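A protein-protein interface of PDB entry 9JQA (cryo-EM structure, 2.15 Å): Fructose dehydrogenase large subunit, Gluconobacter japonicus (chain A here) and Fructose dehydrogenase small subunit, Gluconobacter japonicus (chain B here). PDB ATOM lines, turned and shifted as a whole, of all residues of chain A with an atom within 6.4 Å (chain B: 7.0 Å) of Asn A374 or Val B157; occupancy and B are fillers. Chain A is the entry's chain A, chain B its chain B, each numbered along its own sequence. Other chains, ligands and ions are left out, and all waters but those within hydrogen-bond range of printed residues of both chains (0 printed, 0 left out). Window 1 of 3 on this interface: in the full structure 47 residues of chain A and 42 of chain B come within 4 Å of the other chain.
N of Ala A372 sits at hydrogen-bond distance from OD1 of Asn A220. O of Ala A400 lies within hydrogen-bond range of N of Trp A338 (2.9 Å). OG1 of Thr A399 sits at hydrogen-bond distance from N of Asn A374, 3.4 Å away.
ND2 of Asn A374 is in hydrogen-bond range of O of Val B158, 2.8 Å away. The side-chain hydroxyl of Ser A375 is in hydrogen-bond range of the side-chain hydroxyl of Tyr B150, 2.6 Å away.
Asn A220 touches Val B158. CE3 of Trp A338 touches CG1 of Val B156, 3.5 Å away. Trp A338 touches Val B157. Gly A340 touches Val B158 (O to CG1, 3.4 Å). O of Val B158 touches CB of Ala A372, 3.9 Å away. CB of Asn A374 touches OG of Ser B153, 3.96 Å away. Asn A374 touches Val B157. Met B149 touches Gly A378. Ile A395 touches Met B149. Thr A399 touches Ser B153 (CG2 to CB, 3.4 Å).
Printed residues of chain B within 4 Å of Asn A220: Val B158. Ala A377 touches none of the printed residues of chain B. Printed residues of chain B within 4 Å of Thr A399: Ser B153 and Val B157. Of the printed residues of chain A, Met B149 touches Ser A375, Gly A378 and Ile A395. Printed residues of chain A within 4 Å of Ser B153: Asn A374 and Thr A399. Val B157 touches just these residues of chain A: Trp A338, Ala A339, Ala A372, Asn A374 and Thr A399. Printed residues of chain A within 4 Å of Tyr B169: Gly A340 (3.9 Å). The nearest printed residue of chain B that does not touch Asn A374 is Ile B159 (4.1 Å).
Printed residues of chain B that touch a printed residue of chain A: Met B149, Tyr B150, Ser B153, Val B156, Val B157, Val B158 and Tyr B169. Of the 17 printed residues of chain A, 10 touch a printed residue of chain B. Printed residues of chain A that touch a printed residue of chain B: Asn A220, Trp A338, Ala A339, Gly A340, Ala A372, Asn A374, Ser A375, Gly A378, Ile A395 and Thr A399. Hydrophobic or aromatic side chains of chain A within 4 Å of the printed part of chain B: Trp A338, Ala A372 and Ile A395.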
ATOM      1  N   ASN A 220     -11.020 -26.587  -4.504  1.00  0.00           N
ATOM      2  CA  ASN A 220     -11.993 -27.554  -4.999  1.00  0.00           C
ATOM      3  C   ASN A 220     -11.379 -28.482  -6.041  1.00  0.00           C
ATOM      4  O   ASN A 220     -12.046 -28.910  -6.984  1.00  0.00           O
ATOM      5  CB  ASN A 220     -13.225 -26.844  -5.566  1.00  0.00           C
ATOM      6  CG  ASN A 220     -14.446 -27.725  -5.598  1.00  0.00           C
ATOM      7  OD1 ASN A 220     -15.044 -27.933  -6.649  1.00  0.00           O
ATOM      8  ND2 ASN A 220     -14.828 -28.249  -4.444  1.00  0.00           N
ATOM      9  N   TRP A 338     -25.081 -25.059  -6.135  1.00  0.00           N
ATOM     10  CA  TRP A 338     -23.815 -24.336  -6.255  1.00  0.00           C
ATOM     11  C   TRP A 338     -22.651 -25.139  -5.673  1.00  0.00           C
ATOM     12  O   TRP A 338     -22.010 -24.743  -4.701  1.00  0.00           O
ATOM     13  CB  TRP A 338     -23.906 -22.964  -5.585  1.00  0.00           C
ATOM     14  CG  TRP A 338     -24.848 -21.996  -6.229  1.00  0.00           C
ATOM     15  CD1 TRP A 338     -26.018 -21.537  -5.713  1.00  0.00           C
ATOM     16  CD2 TRP A 338     -24.683 -21.343  -7.492  1.00  0.00           C
ATOM     17  NE1 TRP A 338     -26.598 -20.644  -6.576  1.00  0.00           N
ATOM     18  CE2 TRP A 338     -25.797 -20.508  -7.677  1.00  0.00           C
ATOM     19  CE3 TRP A 338     -23.706 -21.389  -8.487  1.00  0.00           C
ATOM     20  CZ2 TRP A 338     -25.961 -19.725  -8.815  1.00  0.00           C
ATOM     21  CZ3 TRP A 338     -23.869 -20.611  -9.613  1.00  0.00           C
ATOM     22  CH2 TRP A 338     -24.987 -19.790  -9.769  1.00  0.00           C
ATOM     23  N   ALA A 339     -22.388 -26.288  -6.284  1.00  0.00           N
ATOM     24  CA  ALA A 339     -21.269 -27.115  -5.859  1.00  0.00           C
ATOM     25  C   ALA A 339     -19.949 -26.406  -6.126  1.00  0.00           C
ATOM     26  O   ALA A 339     -19.791 -25.713  -7.133  1.00  0.00           O
ATOM     27  CB  ALA A 339     -21.293 -28.459  -6.580  1.00  0.00           C
ATOM     28  N   GLY A 340     -18.996 -26.578  -5.214  1.00  0.00           N
ATOM     29  CA  GLY A 340     -17.677 -26.017  -5.413  1.00  0.00           C
ATOM     30  C   GLY A 340     -17.148 -25.210  -4.247  1.00  0.00           C
ATOM     31  O   GLY A 340     -15.961 -24.883  -4.206  1.00  0.00           O
ATOM     32  N   THR A 371     -17.509 -31.235  -5.822  1.00  0.00           N
ATOM     33  CA  THR A 371     -16.702 -30.753  -6.933  1.00  0.00           C
ATOM     34  C   THR A 371     -17.501 -29.769  -7.776  1.00  0.00           C
ATOM     35  O   THR A 371     -18.682 -29.982  -8.053  1.00  0.00           O
ATOM     36  CB  THR A 371     -16.236 -31.920  -7.801  1.00  0.00           C
ATOM     37  OG1 THR A 371     -15.839 -33.010  -6.962  1.00  0.00           O
ATOM     38  CG2 THR A 371     -15.062 -31.500  -8.665  1.00  0.00           C
ATOM     39  N   ALA A 372     -16.849 -28.681  -8.172  1.00  0.00           N
ATOM     40  CA  ALA A 372     -17.507 -27.671  -8.987  1.00  0.00           C
ATOM     41  C   ALA A 372     -17.999 -28.278 -10.292  1.00  0.00           C
ATOM     42  O   ALA A 372     -17.300 -29.060 -10.939  1.00  0.00           O
ATOM     43  CB  ALA A 372     -16.553 -26.513  -9.269  1.00  0.00           C
ATOM     44  N   GLN A 373     -19.219 -27.911 -10.678  1.00  0.00           N
ATOM     45  CA  GLN A 373     -19.867 -28.462 -11.859  1.00  0.00           C
ATOM     46  C   GLN A 373     -19.784 -27.523 -13.057  1.00  0.00           C
ATOM     47  O   GLN A 373     -20.623 -27.601 -13.957  1.00  0.00           O
ATOM     48  CB  GLN A 373     -21.326 -28.795 -11.551  1.00  0.00           C
ATOM     49  CG  GLN A 373     -21.509 -29.893 -10.523  1.00  0.00           C
ATOM     50  CD  GLN A 373     -22.029 -31.176 -11.131  1.00  0.00           C
ATOM     51  OE1 GLN A 373     -22.742 -31.156 -12.131  1.00  0.00           O
ATOM     52  NE2 GLN A 373     -21.670 -32.300 -10.532  1.00  0.00           N
ATOM     53  N   ASN A 374     -18.791 -26.633 -13.085  1.00  0.00           N
ATOM     54  CA  ASN A 374     -18.699 -25.679 -14.184  1.00  0.00           C
ATOM     55  C   ASN A 374     -18.193 -26.330 -15.465  1.00  0.00           C
ATOM     56  O   ASN A 374     -18.687 -26.017 -16.551  1.00  0.00           O
ATOM     57  CB  ASN A 374     -17.809 -24.498 -13.797  1.00  0.00           C
ATOM     58  CG  ASN A 374     -16.671 -24.897 -12.888  1.00  0.00           C
ATOM     59  OD1 ASN A 374     -16.262 -26.055 -12.856  1.00  0.00           O
ATOM     60  ND2 ASN A 374     -16.147 -23.933 -12.148  1.00  0.00           N
ATOM     61  N   SER A 375     -17.209 -27.225 -15.369  1.00  0.00           N
ATOM     62  CA  SER A 375     -16.753 -27.935 -16.561  1.00  0.00           C
ATOM     63  C   SER A 375     -17.840 -28.851 -17.107  1.00  0.00           C
ATOM     64  O   SER A 375     -18.076 -28.891 -18.321  1.00  0.00           O
ATOM     65  CB  SER A 375     -15.488 -28.734 -16.252  1.00  0.00           C
ATOM     66  OG  SER A 375     -14.454 -27.890 -15.784  1.00  0.00           O
ATOM     67  N   ARG A 376     -18.516 -29.585 -16.223  1.00  0.00           N
ATOM     68  CA  ARG A 376     -19.605 -30.455 -16.648  1.00  0.00           C
ATOM     69  C   ARG A 376     -20.726 -29.652 -17.291  1.00  0.00           C
ATOM     70  O   ARG A 376     -21.234 -30.013 -18.359  1.00  0.00           O
ATOM     71  CB  ARG A 376     -20.124 -31.252 -15.452  1.00  0.00           C
ATOM     72  CG  ARG A 376     -21.386 -32.041 -15.722  1.00  0.00           C
ATOM     73  CD  ARG A 376     -21.072 -33.503 -15.951  1.00  0.00           C
ATOM     74  NE  ARG A 376     -19.993 -33.961 -15.087  1.00  0.00           N
ATOM     75  CZ  ARG A 376     -20.175 -34.545 -13.912  1.00  0.00           C
ATOM     76  NH1 ARG A 376     -21.385 -34.767 -13.430  1.00  0.00           N
ATOM     77  NH2 ARG A 376     -19.114 -34.917 -13.202  1.00  0.00           N
ATOM     78  N   ALA A 377     -21.112 -28.543 -16.657  1.00  0.00           N
ATOM     79  CA  ALA A 377     -22.170 -27.703 -17.203  1.00  0.00           C
ATOM     80  C   ALA A 377     -21.775 -27.120 -18.549  1.00  0.00           C
ATOM     81  O   ALA A 377     -22.582 -27.097 -19.484  1.00  0.00           O
ATOM     82  CB  ALA A 377     -22.506 -26.583 -16.224  1.00  0.00           C
ATOM     83  N   GLY A 378     -20.537 -26.641 -18.666  1.00  0.00           N
ATOM     84  CA  GLY A 378     -20.096 -26.063 -19.921  1.00  0.00           C
ATOM     85  C   GLY A 378     -20.086 -27.073 -21.048  1.00  0.00           C
ATOM     86  O   GLY A 378     -20.579 -26.802 -22.144  1.00  0.00           O
ATOM     87  N   MET A 379     -19.540 -28.262 -20.788  1.00  0.00           N
ATOM     88  CA  MET A 379     -19.502 -29.286 -21.825  1.00  0.00           C
ATOM     89  C   MET A 379     -20.905 -29.733 -22.214  1.00  0.00           C
ATOM     90  O   MET A 379     -21.197 -29.909 -23.402  1.00  0.00           O
ATOM     91  CB  MET A 379     -18.662 -30.474 -21.361  1.00  0.00           C
ATOM     92  CG  MET A 379     -17.199 -30.139 -21.137  1.00  0.00           C
ATOM     93  SD  MET A 379     -16.476 -29.174 -22.475  1.00  0.00           S
ATOM     94  CE  MET A 379     -16.493 -30.364 -23.808  1.00  0.00           C
ATOM     95  N   ILE A 395     -25.319 -22.761 -19.163  1.00  0.00           N
ATOM     96  CA  ILE A 395     -24.108 -23.064 -18.407  1.00  0.00           C
ATOM     97  C   ILE A 395     -24.290 -22.678 -16.946  1.00  0.00           C
ATOM     98  O   ILE A 395     -23.985 -23.458 -16.036  1.00  0.00           O
ATOM     99  CB  ILE A 395     -22.891 -22.356 -19.026  1.00  0.00           C
ATOM    100  CG1 ILE A 395     -22.525 -22.988 -20.365  1.00  0.00           C
ATOM    101  CG2 ILE A 395     -21.708 -22.426 -18.086  1.00  0.00           C
ATOM    102  CD1 ILE A 395     -21.680 -22.103 -21.240  1.00  0.00           C
ATOM    103  N   ARG A 398     -26.865 -25.044 -15.191  1.00  0.00           N
ATOM    104  CA  ARG A 398     -26.388 -26.401 -14.975  1.00  0.00           C
ATOM    105  C   ARG A 398     -25.237 -26.452 -13.981  1.00  0.00           C
ATOM    106  O   ARG A 398     -25.050 -27.476 -13.317  1.00  0.00           O
ATOM    107  CB  ARG A 398     -25.983 -27.031 -16.305  1.00  0.00           C
ATOM    108  CG  ARG A 398     -27.158 -27.298 -17.215  1.00  0.00           C
ATOM    109  CD  ARG A 398     -26.766 -28.143 -18.403  1.00  0.00           C
ATOM    110  NE  ARG A 398     -27.936 -28.751 -19.021  1.00  0.00           N
ATOM    111  CZ  ARG A 398     -28.423 -29.939 -18.694  1.00  0.00           C
ATOM    112  NH1 ARG A 398     -27.849 -30.689 -17.770  1.00  0.00           N
ATOM    113  NH2 ARG A 398     -29.512 -30.384 -19.310  1.00  0.00           N
ATOM    114  N   THR A 399     -24.459 -25.377 -13.855  1.00  0.00           N
ATOM    115  CA  THR A 399     -23.451 -25.354 -12.806  1.00  0.00           C
ATOM    116  C   THR A 399     -24.038 -24.993 -11.449  1.00  0.00           C
ATOM    117  O   THR A 399     -23.453 -25.350 -10.422  1.00  0.00           O
ATOM    118  CB  THR A 399     -22.319 -24.389 -13.167  1.00  0.00           C
ATOM    119  OG1 THR A 399     -21.268 -24.497 -12.200  1.00  0.00           O
ATOM    120  CG2 THR A 399     -22.812 -22.984 -13.173  1.00  0.00           C
ATOM    121  N   ALA A 400     -25.178 -24.300 -11.417  1.00  0.00           N
ATOM    122  CA  ALA A 400     -25.856 -24.046 -10.153  1.00  0.00           C
ATOM    123  C   ALA A 400     -26.650 -25.252  -9.670  1.00  0.00           C
ATOM    124  O   ALA A 400     -26.762 -25.467  -8.460  1.00  0.00           O
ATOM    125  CB  ALA A 400     -26.784 -22.841 -10.287  1.00  0.00           C
ATOM    126  N   PHE B 144      -7.856 -22.026 -20.308  1.00  0.00           N
ATOM    127  CA  PHE B 144      -8.500 -22.347 -19.047  1.00  0.00           C
ATOM    128  C   PHE B 144      -8.593 -21.044 -18.269  1.00  0.00           C
ATOM    129  O   PHE B 144      -7.745 -20.160 -18.416  1.00  0.00           O
ATOM    130  CB  PHE B 144      -7.707 -23.406 -18.264  1.00  0.00           C
ATOM    131  CG  PHE B 144      -8.370 -23.868 -16.997  1.00  0.00           C
ATOM    132  CD1 PHE B 144      -9.627 -24.447 -17.019  1.00  0.00           C
ATOM    133  CD2 PHE B 144      -7.724 -23.738 -15.782  1.00  0.00           C
ATOM    134  CE1 PHE B 144     -10.223 -24.879 -15.854  1.00  0.00           C
ATOM    135  CE2 PHE B 144      -8.316 -24.165 -14.618  1.00  0.00           C
ATOM    136  CZ  PHE B 144      -9.565 -24.738 -14.652  1.00  0.00           C
ATOM    137  N   MET B 149     -16.798 -20.680 -20.940  1.00  0.00           N
ATOM    138  CA  MET B 149     -17.788 -21.484 -20.237  1.00  0.00           C
ATOM    139  C   MET B 149     -17.615 -21.455 -18.726  1.00  0.00           C
ATOM    140  O   MET B 149     -18.484 -21.960 -18.012  1.00  0.00           O
ATOM    141  CB  MET B 149     -17.745 -22.931 -20.733  1.00  0.00           C
ATOM    142  CG  MET B 149     -16.613 -23.757 -20.169  1.00  0.00           C
ATOM    143  SD  MET B 149     -16.601 -25.424 -20.842  1.00  0.00           S
ATOM    144  CE  MET B 149     -15.515 -26.229 -19.680  1.00  0.00           C
ATOM    145  N   TYR B 150     -16.521 -20.889 -18.223  1.00  0.00           N
ATOM    146  CA  TYR B 150     -16.352 -20.698 -16.791  1.00  0.00           C
ATOM    147  C   TYR B 150     -16.791 -19.320 -16.326  1.00  0.00           C
ATOM    148  O   TYR B 150     -16.873 -19.088 -15.117  1.00  0.00           O
ATOM    149  CB  TYR B 150     -14.891 -20.926 -16.394  1.00  0.00           C
ATOM    150  CG  TYR B 150     -14.415 -22.336 -16.626  1.00  0.00           C
ATOM    151  CD1 TYR B 150     -14.861 -23.378 -15.830  1.00  0.00           C
ATOM    152  CD2 TYR B 150     -13.522 -22.627 -17.645  1.00  0.00           C
ATOM    153  CE1 TYR B 150     -14.430 -24.667 -16.040  1.00  0.00           C
ATOM    154  CE2 TYR B 150     -13.086 -23.913 -17.861  1.00  0.00           C
ATOM    155  CZ  TYR B 150     -13.544 -24.930 -17.057  1.00  0.00           C
ATOM    156  OH  TYR B 150     -13.111 -26.216 -17.269  1.00  0.00           O
ATOM    157  N   SER B 153     -20.472 -18.467 -14.361  1.00  0.00           N
ATOM    158  CA  SER B 153     -20.565 -18.812 -12.949  1.00  0.00           C
ATOM    159  C   SER B 153     -19.363 -18.354 -12.137  1.00  0.00           C
ATOM    160  O   SER B 153     -19.200 -18.799 -10.996  1.00  0.00           O
ATOM    161  CB  SER B 153     -20.740 -20.320 -12.787  1.00  0.00           C
ATOM    162  OG  SER B 153     -19.643 -21.020 -13.341  1.00  0.00           O
ATOM    163  N   ARG B 154     -18.520 -17.480 -12.686  1.00  0.00           N
ATOM    164  CA  ARG B 154     -17.316 -17.069 -11.973  1.00  0.00           C
ATOM    165  C   ARG B 154     -17.641 -16.309 -10.696  1.00  0.00           C
ATOM    166  O   ARG B 154     -16.881 -16.376  -9.725  1.00  0.00           O
ATOM    167  CB  ARG B 154     -16.436 -16.211 -12.878  1.00  0.00           C
ATOM    168  CG  ARG B 154     -15.221 -16.929 -13.396  1.00  0.00           C
ATOM    169  CD  ARG B 154     -14.324 -15.987 -14.159  1.00  0.00           C
ATOM    170  NE  ARG B 154     -13.075 -15.739 -13.454  1.00  0.00           N
ATOM    171  CZ  ARG B 154     -11.925 -15.466 -14.052  1.00  0.00           C
ATOM    172  NH1 ARG B 154     -11.833 -15.397 -15.369  1.00  0.00           N
ATOM    173  NH2 ARG B 154     -10.843 -15.258 -13.310  1.00  0.00           N
ATOM    174  N   ASP B 155     -18.755 -15.579 -10.677  1.00  0.00           N
ATOM    175  CA  ASP B 155     -19.110 -14.804  -9.497  1.00  0.00           C
ATOM    176  C   ASP B 155     -19.458 -15.685  -8.306  1.00  0.00           C
ATOM    177  O   ASP B 155     -19.443 -15.199  -7.171  1.00  0.00           O
ATOM    178  CB  ASP B 155     -20.275 -13.869  -9.814  1.00  0.00           C
ATOM    179  CG  ASP B 155     -21.538 -14.617 -10.178  1.00  0.00           C
ATOM    180  OD1 ASP B 155     -21.434 -15.697 -10.791  1.00  0.00           O
ATOM    181  OD2 ASP B 155     -22.635 -14.121  -9.854  1.00  0.00           O
ATOM    182  N   VAL B 156     -19.765 -16.959  -8.531  1.00  0.00           N
ATOM    183  CA  VAL B 156     -20.131 -17.856  -7.443  1.00  0.00           C
ATOM    184  C   VAL B 156     -19.178 -19.042  -7.393  1.00  0.00           C
ATOM    185  O   VAL B 156     -18.565 -19.315  -6.357  1.00  0.00           O
ATOM    186  CB  VAL B 156     -21.584 -18.342  -7.585  1.00  0.00           C
ATOM    187  CG1 VAL B 156     -21.937 -19.256  -6.431  1.00  0.00           C
ATOM    188  CG2 VAL B 156     -22.536 -17.166  -7.647  1.00  0.00           C
ATOM    189  N   VAL B 157     -19.049 -19.750  -8.507  1.00  0.00           N
ATOM    190  CA  VAL B 157     -18.357 -21.033  -8.534  1.00  0.00           C
ATOM    191  C   VAL B 157     -16.883 -20.811  -8.838  1.00  0.00           C
ATOM    192  O   VAL B 157     -16.529 -20.066  -9.758  1.00  0.00           O
ATOM    193  CB  VAL B 157     -18.997 -21.979  -9.560  1.00  0.00           C
ATOM    194  CG1 VAL B 157     -18.245 -23.290  -9.604  1.00  0.00           C
ATOM    195  CG2 VAL B 157     -20.447 -22.217  -9.209  1.00  0.00           C
ATOM    196  N   VAL B 158     -16.025 -21.463  -8.057  1.00  0.00           N
ATOM    197  CA  VAL B 158     -14.586 -21.358  -8.243  1.00  0.00           C
ATOM    198  C   VAL B 158     -14.173 -22.049  -9.534  1.00  0.00           C
ATOM    199  O   VAL B 158     -14.698 -23.111  -9.892  1.00  0.00           O
ATOM    200  CB  VAL B 158     -13.863 -21.971  -7.030  1.00  0.00           C
ATOM    201  CG1 VAL B 158     -14.330 -23.396  -6.803  1.00  0.00           C
ATOM    202  CG2 VAL B 158     -12.368 -21.937  -7.217  1.00  0.00           C
ATOM    203  N   ILE B 159     -13.243 -21.434 -10.257  1.00  0.00           N
ATOM    204  CA  ILE B 159     -12.503 -22.140 -11.297  1.00  0.00           C
ATOM    205  C   ILE B 159     -11.419 -22.916 -10.559  1.00  0.00           C
ATOM    206  O   ILE B 159     -10.514 -22.302  -9.982  1.00  0.00           O
ATOM    207  CB  ILE B 159     -11.923 -21.177 -12.341  1.00  0.00           C
ATOM    208  CG1 ILE B 159     -13.031 -20.304 -12.924  1.00  0.00           C
ATOM    209  CG2 ILE B 159     -11.222 -21.944 -13.436  1.00  0.00           C
ATOM    210  CD1 ILE B 159     -12.559 -19.375 -14.005  1.00  0.00           C
ATOM    211  N   PRO B 160     -11.460 -24.248 -10.569  1.00  0.00           N
ATOM    212  CA  PRO B 160     -10.826 -25.023  -9.493  1.00  0.00           C
ATOM    213  C   PRO B 160      -9.411 -24.642  -9.075  1.00  0.00           C
ATOM    214  O   PRO B 160      -9.230 -24.212  -7.935  1.00  0.00           O
ATOM    215  CB  PRO B 160     -10.884 -26.446 -10.051  1.00  0.00           C
ATOM    216  CG  PRO B 160     -12.200 -26.443 -10.743  1.00  0.00           C
ATOM    217  CD  PRO B 160     -12.211 -25.126 -11.481  1.00  0.00           C
ATOM    218  N   HIS B 164     -11.073 -18.500  -5.633  1.00  0.00           N
ATOM    219  CA  HIS B 164     -12.145 -17.525  -5.813  1.00  0.00           C
ATOM    220  C   HIS B 164     -11.881 -16.258  -5.000  1.00  0.00           C
ATOM    221  O   HIS B 164     -11.911 -15.145  -5.536  1.00  0.00           O
ATOM    222  CB  HIS B 164     -13.479 -18.168  -5.428  1.00  0.00           C
ATOM    223  CG  HIS B 164     -14.679 -17.407  -5.892  1.00  0.00           C
ATOM    224  ND1 HIS B 164     -15.475 -16.682  -5.034  1.00  0.00           N
ATOM    225  CD2 HIS B 164     -15.231 -17.274  -7.121  1.00  0.00           C
ATOM    226  CE1 HIS B 164     -16.457 -16.123  -5.715  1.00  0.00           C
ATOM    227  NE2 HIS B 164     -16.333 -16.467  -6.984  1.00  0.00           N
ATOM    228  N   TYR B 169     -14.394 -18.210   2.194  1.00  0.00           N
ATOM    229  CA  TYR B 169     -15.384 -17.375   1.529  1.00  0.00           C
ATOM    230  C   TYR B 169     -16.741 -18.040   1.415  1.00  0.00           C
ATOM    231  O   TYR B 169     -17.766 -17.353   1.353  1.00  0.00           O
ATOM    232  CB  TYR B 169     -14.878 -17.011   0.148  1.00  0.00           C
ATOM    233  CG  TYR B 169     -14.920 -18.114  -0.904  1.00  0.00           C
ATOM    234  CD1 TYR B 169     -16.071 -18.379  -1.638  1.00  0.00           C
ATOM    235  CD2 TYR B 169     -13.790 -18.873  -1.179  1.00  0.00           C
ATOM    236  CE1 TYR B 169     -16.092 -19.368  -2.603  1.00  0.00           C
ATOM    237  CE2 TYR B 169     -13.803 -19.859  -2.143  1.00  0.00           C
ATOM    238  CZ  TYR B 169     -14.956 -20.102  -2.852  1.00  0.00           C
ATOM    239  OH  TYR B 169     -14.987 -21.080  -3.814  1.00  0.00           O
